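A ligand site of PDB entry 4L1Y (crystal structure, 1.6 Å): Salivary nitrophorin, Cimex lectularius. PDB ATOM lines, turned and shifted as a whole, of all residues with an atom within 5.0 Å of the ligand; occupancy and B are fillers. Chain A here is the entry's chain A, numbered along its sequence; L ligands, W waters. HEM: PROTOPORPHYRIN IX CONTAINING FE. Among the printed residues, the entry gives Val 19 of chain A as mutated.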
ATOM      1  N   TRP A  12      10.473 -26.978 -33.993  1.00  0.00           N
ATOM      2  CA  TRP A  12      11.666 -27.785 -33.693  1.00  0.00           C
ATOM      3  C   TRP A  12      11.275 -29.206 -33.288  1.00  0.00           C
ATOM      4  O   TRP A  12      10.440 -29.352 -32.382  1.00  0.00           O
ATOM      5  CB  TRP A  12      12.403 -27.139 -32.517  1.00  0.00           C
ATOM      6  CG  TRP A  12      13.802 -27.576 -32.220  1.00  0.00           C
ATOM      7  CD1 TRP A  12      14.630 -28.360 -32.977  1.00  0.00           C
ATOM      8  CD2 TRP A  12      14.615 -27.111 -31.115  1.00  0.00           C
ATOM      9  NE1 TRP A  12      15.879 -28.457 -32.390  1.00  0.00           N
ATOM     10  CE2 TRP A  12      15.898 -27.669 -31.264  1.00  0.00           C
ATOM     11  CE3 TRP A  12      14.359 -26.273 -30.042  1.00  0.00           C
ATOM     12  CZ2 TRP A  12      16.946 -27.436 -30.337  1.00  0.00           C
ATOM     13  CZ3 TRP A  12      15.362 -26.036 -29.111  1.00  0.00           C
ATOM     14  CH2 TRP A  12      16.662 -26.594 -29.283  1.00  0.00           C
ATOM     15  N   SER A  14      12.438 -31.340 -31.258  1.00  0.00           N
ATOM     16  CA  SER A  14      13.325 -31.108 -30.089  1.00  0.00           C
ATOM     17  C   SER A  14      13.650 -32.346 -29.205  1.00  0.00           C
ATOM     18  O   SER A  14      14.667 -32.343 -28.459  1.00  0.00           O
ATOM     19  CB  SER A  14      12.716 -29.986 -29.197  1.00  0.00           C
ATOM     20  OG  SER A  14      11.442 -30.301 -28.921  1.00  0.00           O
ATOM     21  N   GLY A  15      12.888 -33.392 -29.406  1.00  0.00           N
ATOM     22  CA  GLY A  15      13.078 -34.679 -28.661  1.00  0.00           C
ATOM     23  C   GLY A  15      12.961 -34.492 -27.159  1.00  0.00           C
ATOM     24  O   GLY A  15      11.923 -34.095 -26.712  1.00  0.00           O
ATOM     25  N   HIS A  16      14.025 -34.755 -26.420  1.00  0.00           N
ATOM     26  CA  HIS A  16      14.072 -34.525 -24.950  1.00  0.00           C
ATOM     27  C   HIS A  16      14.647 -33.180 -24.537  1.00  0.00           C
ATOM     28  O   HIS A  16      14.823 -32.933 -23.321  1.00  0.00           O
ATOM     29  CB  HIS A  16      14.919 -35.613 -24.259  1.00  0.00           C
ATOM     30  CG  HIS A  16      14.396 -36.979 -24.446  1.00  0.00           C
ATOM     31  ND1 HIS A  16      15.050 -37.916 -25.216  1.00  0.00           N
ATOM     32  CD2 HIS A  16      13.262 -37.580 -24.009  1.00  0.00           C
ATOM     33  CE1 HIS A  16      14.344 -39.036 -25.258  1.00  0.00           C
ATOM     34  NE2 HIS A  16      13.249 -38.857 -24.536  1.00  0.00           N
ATOM     35  N   GLU A  17      15.011 -32.323 -25.507  1.00  0.00           N
ATOM     36  CA  GLU A  17      15.557 -31.021 -25.151  1.00  0.00           C
ATOM     37  C   GLU A  17      14.583 -30.197 -24.339  1.00  0.00           C
ATOM     38  O   GLU A  17      13.396 -30.038 -24.709  1.00  0.00           O
ATOM     39  CB  GLU A  17      15.977 -30.217 -26.385  1.00  0.00           C
ATOM     40  CG  GLU A  17      17.278 -30.752 -26.970  1.00  0.00           C
ATOM     41  CD  GLU A  17      18.381 -30.886 -25.907  1.00  0.00           C
ATOM     42  OE1 GLU A  17      18.738 -29.882 -25.266  1.00  0.00           O
ATOM     43  OE2 GLU A  17      18.921 -31.992 -25.743  1.00  0.00           O
ATOM     44  N   ARG A  18      15.145 -29.563 -23.311  1.00  0.00           N
ATOM     45  CA  ARG A  18      14.425 -28.524 -22.559  1.00  0.00           C
ATOM     46  C   ARG A  18      14.463 -27.224 -23.343  1.00  0.00           C
ATOM     47  O   ARG A  18      15.280 -27.041 -24.217  1.00  0.00           O
ATOM     48  CB  ARG A  18      15.064 -28.304 -21.201  1.00  0.00           C
ATOM     49  CG  ARG A  18      15.459 -29.597 -20.528  1.00  0.00           C
ATOM     50  CD  ARG A  18      16.198 -29.302 -19.228  1.00  0.00           C
ATOM     51  NE  ARG A  18      15.186 -29.198 -18.243  1.00  0.00           N
ATOM     52  CZ  ARG A  18      14.614 -30.252 -17.672  1.00  0.00           C
ATOM     53  NH1 ARG A  18      15.018 -31.458 -18.001  1.00  0.00           N
ATOM     54  NH2 ARG A  18      13.628 -30.071 -16.813  1.00  0.00           N
ATOM     55  N   VAL A  19      13.613 -26.278 -22.960  1.00  0.00           N
ATOM     56  CA  VAL A  19      13.688 -24.899 -23.509  1.00  0.00           C
ATOM     57  C   VAL A  19      15.120 -24.327 -23.445  1.00  0.00           C
ATOM     58  O   VAL A  19      15.783 -24.381 -22.386  1.00  0.00           O
ATOM     59  CB  VAL A  19      12.627 -24.035 -22.810  1.00  0.00           C
ATOM     60  CG1 VAL A  19      12.758 -22.554 -23.145  1.00  0.00           C
ATOM     61  CG2 VAL A  19      11.238 -24.498 -23.066  1.00  0.00           C
ATOM     62  N   PRO A  20      15.633 -23.759 -24.541  1.00  0.00           N
ATOM     63  CA  PRO A  20      16.974 -23.191 -24.541  1.00  0.00           C
ATOM     64  C   PRO A  20      17.066 -21.782 -23.929  1.00  0.00           C
ATOM     65  O   PRO A  20      16.041 -21.187 -23.565  1.00  0.00           O
ATOM     66  CB  PRO A  20      17.347 -23.131 -26.039  1.00  0.00           C
ATOM     67  CG  PRO A  20      16.070 -23.197 -26.779  1.00  0.00           C
ATOM     68  CD  PRO A  20      15.076 -23.887 -25.909  1.00  0.00           C
ATOM     69  N   LEU A  26      15.416 -17.604 -30.971  1.00  0.00           N
ATOM     70  CA  LEU A  26      14.527 -18.685 -31.391  1.00  0.00           C
ATOM     71  C   LEU A  26      13.236 -18.160 -32.050  1.00  0.00           C
ATOM     72  O   LEU A  26      12.738 -18.739 -32.998  1.00  0.00           O
ATOM     73  CB  LEU A  26      14.211 -19.613 -30.199  1.00  0.00           C
ATOM     74  CG  LEU A  26      13.440 -20.909 -30.566  1.00  0.00           C
ATOM     75  CD1 LEU A  26      14.413 -21.874 -31.200  1.00  0.00           C
ATOM     76  CD2 LEU A  26      12.826 -21.608 -29.370  1.00  0.00           C
ATOM     77  N   VAL A  40       4.857 -21.149 -31.977  1.00  0.00           N
ATOM     78  CA  VAL A  40       5.926 -22.053 -31.619  1.00  0.00           C
ATOM     79  C   VAL A  40       5.389 -23.525 -31.532  1.00  0.00           C
ATOM     80  O   VAL A  40       4.381 -23.838 -30.795  1.00  0.00           O
ATOM     81  CB  VAL A  40       6.425 -21.719 -30.201  1.00  0.00           C
ATOM     82  CG1 VAL A  40       7.557 -22.647 -29.755  1.00  0.00           C
ATOM     83  CG2 VAL A  40       6.817 -20.249 -30.069  1.00  0.00           C
ATOM     84  N   VAL A  42       6.604 -27.737 -31.287  1.00  0.00           N
ATOM     85  CA  VAL A  42       7.552 -28.781 -31.016  1.00  0.00           C
ATOM     86  C   VAL A  42       7.020 -30.159 -31.305  1.00  0.00           C
ATOM     87  O   VAL A  42       5.826 -30.386 -31.239  1.00  0.00           O
ATOM     88  CB  VAL A  42       8.204 -28.635 -29.547  1.00  0.00           C
ATOM     89  CG1 VAL A  42       9.032 -27.333 -29.433  1.00  0.00           C
ATOM     90  CG2 VAL A  42       7.177 -28.958 -28.399  1.00  0.00           C
ATOM     91  N   PHE A  45       9.326 -36.024 -26.964  1.00  0.00           N
ATOM     92  CA  PHE A  45       8.903 -37.154 -26.083  1.00  0.00           C
ATOM     93  C   PHE A  45       8.462 -36.643 -24.715  1.00  0.00           C
ATOM     94  O   PHE A  45       9.205 -35.927 -23.991  1.00  0.00           O
ATOM     95  CB  PHE A  45      10.112 -38.083 -25.912  1.00  0.00           C
ATOM     96  CG  PHE A  45      10.837 -38.407 -27.216  1.00  0.00           C
ATOM     97  CD1 PHE A  45      12.153 -38.018 -27.426  1.00  0.00           C
ATOM     98  CD2 PHE A  45      10.167 -39.099 -28.234  1.00  0.00           C
ATOM     99  CE1 PHE A  45      12.812 -38.343 -28.595  1.00  0.00           C
ATOM    100  CE2 PHE A  45      10.803 -39.407 -29.427  1.00  0.00           C
ATOM    101  CZ  PHE A  45      12.134 -39.035 -29.601  1.00  0.00           C
ATOM    102  N   GLY A  46       7.248 -36.974 -24.355  1.00  0.00           N
ATOM    103  CA  GLY A  46       6.902 -36.951 -22.931  1.00  0.00           C
ATOM    104  C   GLY A  46       6.356 -35.648 -22.440  1.00  0.00           C
ATOM    105  O   GLY A  46       6.429 -35.357 -21.261  1.00  0.00           O
ATOM    106  N   PHE A  47       5.835 -34.809 -23.322  1.00  0.00           N
ATOM    107  CA  PHE A  47       5.540 -33.455 -22.897  1.00  0.00           C
ATOM    108  C   PHE A  47       4.430 -33.416 -21.825  1.00  0.00           C
ATOM    109  O   PHE A  47       4.581 -32.746 -20.799  1.00  0.00           O
ATOM    110  CB  PHE A  47       5.126 -32.605 -24.093  1.00  0.00           C
ATOM    111  CG  PHE A  47       6.207 -32.403 -25.118  1.00  0.00           C
ATOM    112  CD1 PHE A  47       6.000 -32.797 -26.428  1.00  0.00           C
ATOM    113  CD2 PHE A  47       7.415 -31.778 -24.804  1.00  0.00           C
ATOM    114  CE1 PHE A  47       7.005 -32.549 -27.377  1.00  0.00           C
ATOM    115  CE2 PHE A  47       8.451 -31.550 -25.749  1.00  0.00           C
ATOM    116  CZ  PHE A  47       8.237 -31.977 -27.047  1.00  0.00           C
ATOM    117  N   GLN A  48       3.335 -34.077 -22.096  1.00  0.00           N
ATOM    118  CA  GLN A  48       2.132 -34.008 -21.271  1.00  0.00           C
ATOM    119  C   GLN A  48       2.409 -34.608 -19.872  1.00  0.00           C
ATOM    120  O   GLN A  48       2.029 -33.994 -18.856  1.00  0.00           O
ATOM    121  CB  GLN A  48       0.955 -34.686 -21.996  1.00  0.00           C
ATOM    122  CG  GLN A  48      -0.400 -34.626 -21.268  1.00  0.00           C
ATOM    123  CD  GLN A  48      -1.523 -35.291 -22.068  1.00  0.00           C
ATOM    124  OE1 GLN A  48      -1.343 -35.710 -23.228  1.00  0.00           O
ATOM    125  NE2 GLN A  48      -2.675 -35.420 -21.444  1.00  0.00           N
ATOM    126  N   ASP A  50       5.161 -34.846 -18.443  1.00  0.00           N
ATOM    127  CA  ASP A  50       6.183 -33.976 -17.866  1.00  0.00           C
ATOM    128  C   ASP A  50       6.989 -34.583 -16.658  1.00  0.00           C
ATOM    129  O   ASP A  50       7.120 -33.944 -15.629  1.00  0.00           O
ATOM    130  CB  ASP A  50       5.528 -32.631 -17.485  1.00  0.00           C
ATOM    131  CG  ASP A  50       6.531 -31.534 -17.295  1.00  0.00           C
ATOM    132  OD1 ASP A  50       6.129 -30.423 -16.794  1.00  0.00           O
ATOM    133  OD2 ASP A  50       7.692 -31.781 -17.627  1.00  0.00           O
ATOM    134  N   PRO A  52      10.201 -34.750 -16.485  1.00  0.00           N
ATOM    135  CA  PRO A  52      11.297 -33.799 -16.243  1.00  0.00           C
ATOM    136  C   PRO A  52      10.852 -32.557 -15.432  1.00  0.00           C
ATOM    137  O   PRO A  52      11.715 -31.781 -15.071  1.00  0.00           O
ATOM    138  CB  PRO A  52      11.761 -33.424 -17.671  1.00  0.00           C
ATOM    139  CG  PRO A  52      11.380 -34.639 -18.480  1.00  0.00           C
ATOM    140  CD  PRO A  52      10.055 -35.019 -17.931  1.00  0.00           C
ATOM    141  N   GLN A  54       9.408 -29.936 -16.380  1.00  0.00           N
ATOM    142  CA  GLN A  54       9.972 -28.872 -17.241  1.00  0.00           C
ATOM    143  C   GLN A  54       8.988 -27.764 -17.509  1.00  0.00           C
ATOM    144  O   GLN A  54       9.403 -26.612 -17.705  1.00  0.00           O
ATOM    145  CB  GLN A  54      10.371 -29.449 -18.613  1.00  0.00           C
ATOM    146  CG  GLN A  54      10.682 -28.424 -19.669  1.00  0.00           C
ATOM    147  CD  GLN A  54      11.747 -27.423 -19.292  1.00  0.00           C
ATOM    148  OE1 GLN A  54      12.653 -27.716 -18.483  1.00  0.00           O
ATOM    149  NE2 GLN A  54      11.669 -26.207 -19.874  1.00  0.00           N
ATOM    150  N   GLY A  55       7.718 -28.131 -17.525  1.00  0.00           N
ATOM    151  CA  GLY A  55       6.567 -27.267 -17.924  1.00  0.00           C
ATOM    152  C   GLY A  55       6.506 -25.982 -17.147  1.00  0.00           C
ATOM    153  O   GLY A  55       6.145 -24.937 -17.671  1.00  0.00           O
ATOM    154  N   CYS A  58       9.108 -23.703 -18.714  1.00  0.00           N
ATOM    155  CA  CYS A  58       8.605 -23.206 -20.031  1.00  0.00           C
ATOM    156  C   CYS A  58       7.722 -21.996 -19.856  1.00  0.00           C
ATOM    157  O   CYS A  58       7.913 -20.973 -20.547  1.00  0.00           O
ATOM    158  CB  CYS A  58       7.823 -24.259 -20.824  1.00  0.00           C
ATOM    159  SG  CYS A  58       8.727 -25.817 -21.156  1.00  0.00           S
ATOM    160  N   VAL A  59       6.773 -22.123 -18.934  1.00  0.00           N
ATOM    161  CA  VAL A  59       5.913 -21.013 -18.598  1.00  0.00           C
ATOM    162  C   VAL A  59       6.759 -19.772 -18.188  1.00  0.00           C
ATOM    163  O   VAL A  59       6.612 -18.632 -18.767  1.00  0.00           O
ATOM    164  CB  VAL A  59       4.873 -21.414 -17.539  1.00  0.00           C
ATOM    165  CG1 VAL A  59       4.025 -20.211 -17.141  1.00  0.00           C
ATOM    166  CG2 VAL A  59       3.914 -22.469 -18.067  1.00  0.00           C
ATOM    167  N   PHE A  62       8.793 -18.263 -21.075  1.00  0.00           N
ATOM    168  CA  PHE A  62       8.041 -17.587 -22.174  1.00  0.00           C
ATOM    169  C   PHE A  62       7.245 -16.379 -21.688  1.00  0.00           C
ATOM    170  O   PHE A  62       7.136 -15.392 -22.452  1.00  0.00           O
ATOM    171  CB  PHE A  62       7.205 -18.569 -22.987  1.00  0.00           C
ATOM    172  CG  PHE A  62       8.022 -19.345 -24.002  1.00  0.00           C
ATOM    173  CD1 PHE A  62       8.571 -20.607 -23.687  1.00  0.00           C
ATOM    174  CD2 PHE A  62       8.266 -18.820 -25.279  1.00  0.00           C
ATOM    175  CE1 PHE A  62       9.330 -21.312 -24.603  1.00  0.00           C
ATOM    176  CE2 PHE A  62       9.008 -19.550 -26.216  1.00  0.00           C
ATOM    177  CZ  PHE A  62       9.567 -20.766 -25.876  1.00  0.00           C
ATOM    178  N   GLN A  63       6.731 -16.415 -20.460  1.00  0.00           N
ATOM    179  CA  GLN A  63       6.155 -15.212 -19.802  1.00  0.00           C
ATOM    180  C   GLN A  63       7.182 -14.123 -19.527  1.00  0.00           C
ATOM    181  O   GLN A  63       6.941 -12.967 -19.836  1.00  0.00           O
ATOM    182  CB  GLN A  63       5.329 -15.572 -18.523  1.00  0.00           C
ATOM    183  CG  GLN A  63       6.129 -15.900 -17.254  1.00  0.00           C
ATOM    184  CD  GLN A  63       5.503 -15.435 -15.904  1.00  0.00           C
ATOM    185  OE1 GLN A  63       4.461 -14.794 -15.852  1.00  0.00           O
ATOM    186  NE2 GLN A  63       6.171 -15.767 -14.822  1.00  0.00           N
ATOM    187  N   LYS A  73      -0.719 -15.049 -24.411  1.00  0.00           N
ATOM    188  CA  LYS A  73      -0.766 -16.445 -24.861  1.00  0.00           C
ATOM    189  C   LYS A  73      -2.149 -16.778 -25.153  1.00  0.00           C
ATOM    190  O   LYS A  73      -2.974 -16.860 -24.239  1.00  0.00           O
ATOM    191  CB  LYS A  73      -0.242 -17.393 -23.780  1.00  0.00           C
ATOM    192  CG  LYS A  73      -0.262 -18.853 -24.221  1.00  0.00           C
ATOM    193  CD  LYS A  73       0.073 -19.711 -23.003  1.00  0.00           C
ATOM    194  CE  LYS A  73      -1.190 -20.006 -22.192  1.00  0.00           C
ATOM    195  NZ  LYS A  73      -0.723 -20.780 -21.018  1.00  0.00           N
ATOM    196  N   ASN A  76      -1.755 -22.765 -25.304  1.00  0.00           N
ATOM    197  CA  ASN A  76      -0.701 -23.774 -25.269  1.00  0.00           C
ATOM    198  C   ASN A  76      -1.389 -25.129 -25.208  1.00  0.00           C
ATOM    199  O   ASN A  76      -2.267 -25.296 -24.376  1.00  0.00           O
ATOM    200  CB  ASN A  76       0.212 -23.660 -24.040  1.00  0.00           C
ATOM    201  CG  ASN A  76       1.090 -24.892 -23.866  1.00  0.00           C
ATOM    202  OD1 ASN A  76       0.788 -25.798 -23.034  1.00  0.00           O
ATOM    203  ND2 ASN A  76       2.159 -24.972 -24.673  1.00  0.00           N
ATOM    204  N   ILE A  78      -0.174 -29.393 -25.318  1.00  0.00           N
ATOM    205  CA  ILE A  78       0.812 -30.414 -25.443  1.00  0.00           C
ATOM    206  C   ILE A  78       0.185 -31.793 -25.401  1.00  0.00           C
ATOM    207  O   ILE A  78      -0.828 -32.026 -24.734  1.00  0.00           O
ATOM    208  CB  ILE A  78       1.889 -30.340 -24.334  1.00  0.00           C
ATOM    209  CG1 ILE A  78       1.296 -30.798 -22.980  1.00  0.00           C
ATOM    210  CG2 ILE A  78       2.581 -28.954 -24.374  1.00  0.00           C
ATOM    211  CD1 ILE A  78       1.611 -29.969 -21.793  1.00  0.00           C
ATOM    212  N   THR A  85       2.005 -23.538 -29.300  1.00  0.00           N
ATOM    213  CA  THR A  85       1.624 -22.297 -28.591  1.00  0.00           C
ATOM    214  C   THR A  85       1.437 -21.148 -29.639  1.00  0.00           C
ATOM    215  O   THR A  85       2.255 -20.969 -30.566  1.00  0.00           O
ATOM    216  CB  THR A  85       2.637 -21.948 -27.530  1.00  0.00           C
ATOM    217  OG1 THR A  85       2.984 -23.099 -26.733  1.00  0.00           O
ATOM    218  CG2 THR A  85       2.126 -20.824 -26.596  1.00  0.00           C
ATOM    219  N   TYR A  87       0.706 -17.005 -29.729  1.00  0.00           N
ATOM    220  CA  TYR A  87       0.674 -15.676 -29.077  1.00  0.00           C
ATOM    221  C   TYR A  87       0.227 -14.621 -30.075  1.00  0.00           C
ATOM    222  O   TYR A  87       0.579 -14.628 -31.271  1.00  0.00           O
ATOM    223  CB  TYR A  87       2.040 -15.269 -28.553  1.00  0.00           C
ATOM    224  CG  TYR A  87       2.714 -16.250 -27.583  1.00  0.00           C
ATOM    225  CD1 TYR A  87       3.615 -17.209 -28.051  1.00  0.00           C
ATOM    226  CD2 TYR A  87       2.482 -16.211 -26.165  1.00  0.00           C
ATOM    227  CE1 TYR A  87       4.269 -18.118 -27.190  1.00  0.00           C
ATOM    228  CE2 TYR A  87       3.121 -17.119 -25.314  1.00  0.00           C
ATOM    229  CZ  TYR A  87       4.012 -18.067 -25.806  1.00  0.00           C
ATOM    230  OH  TYR A  87       4.730 -18.970 -24.986  1.00  0.00           O
HETATM  231  CHA HEM L   1       4.710 -25.310 -22.101  1.00  0.00           C
HETATM  232  CHB HEM L   1       8.067 -24.559 -25.476  1.00  0.00           C
HETATM  233  CHC HEM L   1      10.446 -28.487 -24.013  1.00  0.00           C
HETATM  234  CHD HEM L   1       6.744 -29.635 -21.112  1.00  0.00           C
HETATM  235  C1A HEM L   1       5.446 -24.746 -23.102  1.00  0.00           C
HETATM  236  C2A HEM L   1       5.092 -23.548 -23.809  1.00  0.00           C
HETATM  237  C3A HEM L   1       6.028 -23.360 -24.772  1.00  0.00           C
HETATM  238  C4A HEM L   1       6.972 -24.429 -24.652  1.00  0.00           C
HETATM  239  CMA HEM L   1       6.104 -22.177 -25.774  1.00  0.00           C
HETATM  240  CAA HEM L   1       3.945 -22.569 -23.503  1.00  0.00           C
HETATM  241  CBA HEM L   1       4.662 -21.447 -22.685  1.00  0.00           C
HETATM  242  CGA HEM L   1       3.792 -20.393 -22.029  1.00  0.00           C
HETATM  243  O1A HEM L   1       3.083 -20.671 -20.994  1.00  0.00           O
HETATM  244  O2A HEM L   1       3.745 -19.242 -22.538  1.00  0.00           O
HETATM  245  C1B HEM L   1       8.997 -25.591 -25.399  1.00  0.00           C
HETATM  246  C2B HEM L   1      10.143 -25.656 -26.273  1.00  0.00           C
HETATM  247  C3B HEM L   1      10.818 -26.802 -25.885  1.00  0.00           C
HETATM  248  C4B HEM L   1      10.067 -27.351 -24.738  1.00  0.00           C
HETATM  249  CMB HEM L   1      10.518 -24.708 -27.415  1.00  0.00           C
HETATM  250  CAB HEM L   1      12.070 -27.422 -26.264  1.00  0.00           C
HETATM  251  CBB HEM L   1      12.950 -26.883 -27.079  1.00  0.00           C
HETATM  252  C1C HEM L   1       9.644 -29.148 -23.078  1.00  0.00           C
HETATM  253  C2C HEM L   1       9.935 -30.449 -22.573  1.00  0.00           C
HETATM  254  C3C HEM L   1       8.887 -30.778 -21.751  1.00  0.00           C
HETATM  255  C4C HEM L   1       7.938 -29.695 -21.780  1.00  0.00           C
HETATM  256  CMC HEM L   1      11.208 -31.220 -22.880  1.00  0.00           C
HETATM  257  CAC HEM L   1       8.685 -32.010 -20.942  1.00  0.00           C
HETATM  258  CBC HEM L   1       9.368 -33.148 -21.101  1.00  0.00           C
HETATM  259  C1D HEM L   1       5.882 -28.530 -21.200  1.00  0.00           C
HETATM  260  C2D HEM L   1       4.614 -28.536 -20.448  1.00  0.00           C
HETATM  261  C3D HEM L   1       4.044 -27.345 -20.736  1.00  0.00           C
HETATM  262  C4D HEM L   1       4.976 -26.620 -21.622  1.00  0.00           C
HETATM  263  CMD HEM L   1       4.017 -29.644 -19.568  1.00  0.00           C
HETATM  264  CAD HEM L   1       2.712 -26.874 -20.199  1.00  0.00           C
HETATM  265  CBD HEM L   1       3.039 -25.796 -19.155  1.00  0.00           C
HETATM  266  CGD HEM L   1       1.870 -25.297 -18.400  1.00  0.00           C
HETATM  267  O1D HEM L   1       1.893 -25.433 -17.118  1.00  0.00           O
HETATM  268  O2D HEM L   1       0.947 -24.687 -19.042  1.00  0.00           O
HETATM  269  NA  HEM L   1       6.653 -25.220 -23.571  1.00  0.00           N
HETATM  270  NB  HEM L   1       9.087 -26.510 -24.423  1.00  0.00           N
HETATM  271  NC  HEM L   1       8.492 -28.701 -22.519  1.00  0.00           N
HETATM  272  ND  HEM L   1       6.158 -27.303 -21.802  1.00  0.00           N
HETATM  273 FE   HEM L   1       7.569 -26.896 -22.998  1.00  0.00          FE
HETATM  274  O   HOH W   1       6.023 -29.070 -25.170  1.00  0.00           O
HETATM  275  O   HOH W   2      -0.782 -22.952 -17.920  1.00  0.00           O
HETATM  276  O   HOH W   3      -0.704 -25.595 -20.958  1.00  0.00           O
HETATM  277  O   HOH W   4       3.677 -26.983 -15.806  1.00  0.00           O
HETATM  278  O   HOH W   5       1.267 -22.665 -21.080  1.00  0.00           O
HETATM  279  O   HOH W   6       4.749 -26.547 -26.208  1.00  0.00           O
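OH of Tyr 87 sits at hydrogen-bond distance from O2A of the ligand (2.7 Å). NZ of Lys 73 lies within salt-bridge range of O1A of the ligand, at 3.8 Å. SG of Cys 58 is bound to FE of the ligand, at 2.4 Å.
The backbone NH of Gln 54 is in hydrogen-bond range of the side-chain carboxylate of Asp 50 (2.8 Å). ND2 of Asn 76 sits at hydrogen-bond distance from OG1 of Thr 85, at 2.9 Å. N of Gly 55 sits at hydrogen-bond distance from OD1 of Asp 50, at 2.9 Å. The backbone carbonyl oxygen (O) of Pro 52 is in hydrogen-bond range of the guanidinium group (NH2) of Arg 18 (3.1 Å). NE of Arg 18 sits at hydrogen-bond distance from OE1 of Gln 54, at 2.9 Å. SG of Cys 58 lies close to NE2 of Gln 54 (3.2 Å). The backbone NH (N) of Thr 85 is in hydrogen-bond range of the backbone carbonyl oxygen (O) of Val 40.
Merely in contact with the ligand: Trp 12 (3.3 Å), Ser 14 (3.8 Å), Glu 17 (3.1 Å), Arg 18 (3.7 Å), Val 19 (3.2 Å), Pro 20 (3.9 Å), Val 42 (3.6 Å), Gly 46 (3.7 Å), Phe 47 (3.4 Å), Asp 50 (3.5 Å), Pro 52 (3.6 Å), Gln 54 (3.6 Å), Gly 55 (3.4 Å), Val 59 (3.5 Å), Phe 62 (3.5 Å), Asn 76 (3.2 Å), Ile 78 (3.3 Å) and Thr 85 (3.4 Å). Hydrophobic or aromatic side chains within 4 Å of the ligand: Trp 12, Val 19, Pro 20, Val 42, Phe 47, Pro 52, Val 59, Phe 62, Ile 78 and Tyr 87. Of the 28 residues printed, 21 come within 4 Å of the ligand. Along chain A the residues within 4 Å of the ligand span positions 12 to 87.
Water W3 bridges OD1 of Asn 76 (2.6 Å) and O2D of the ligand (2.7 Å). Water W5 lies within hydrogen-bond range of an oxygen (O1A) of the ligand (2.7 Å) and the side-chain amino group (NZ) of Lys 73 (2.7 Å).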
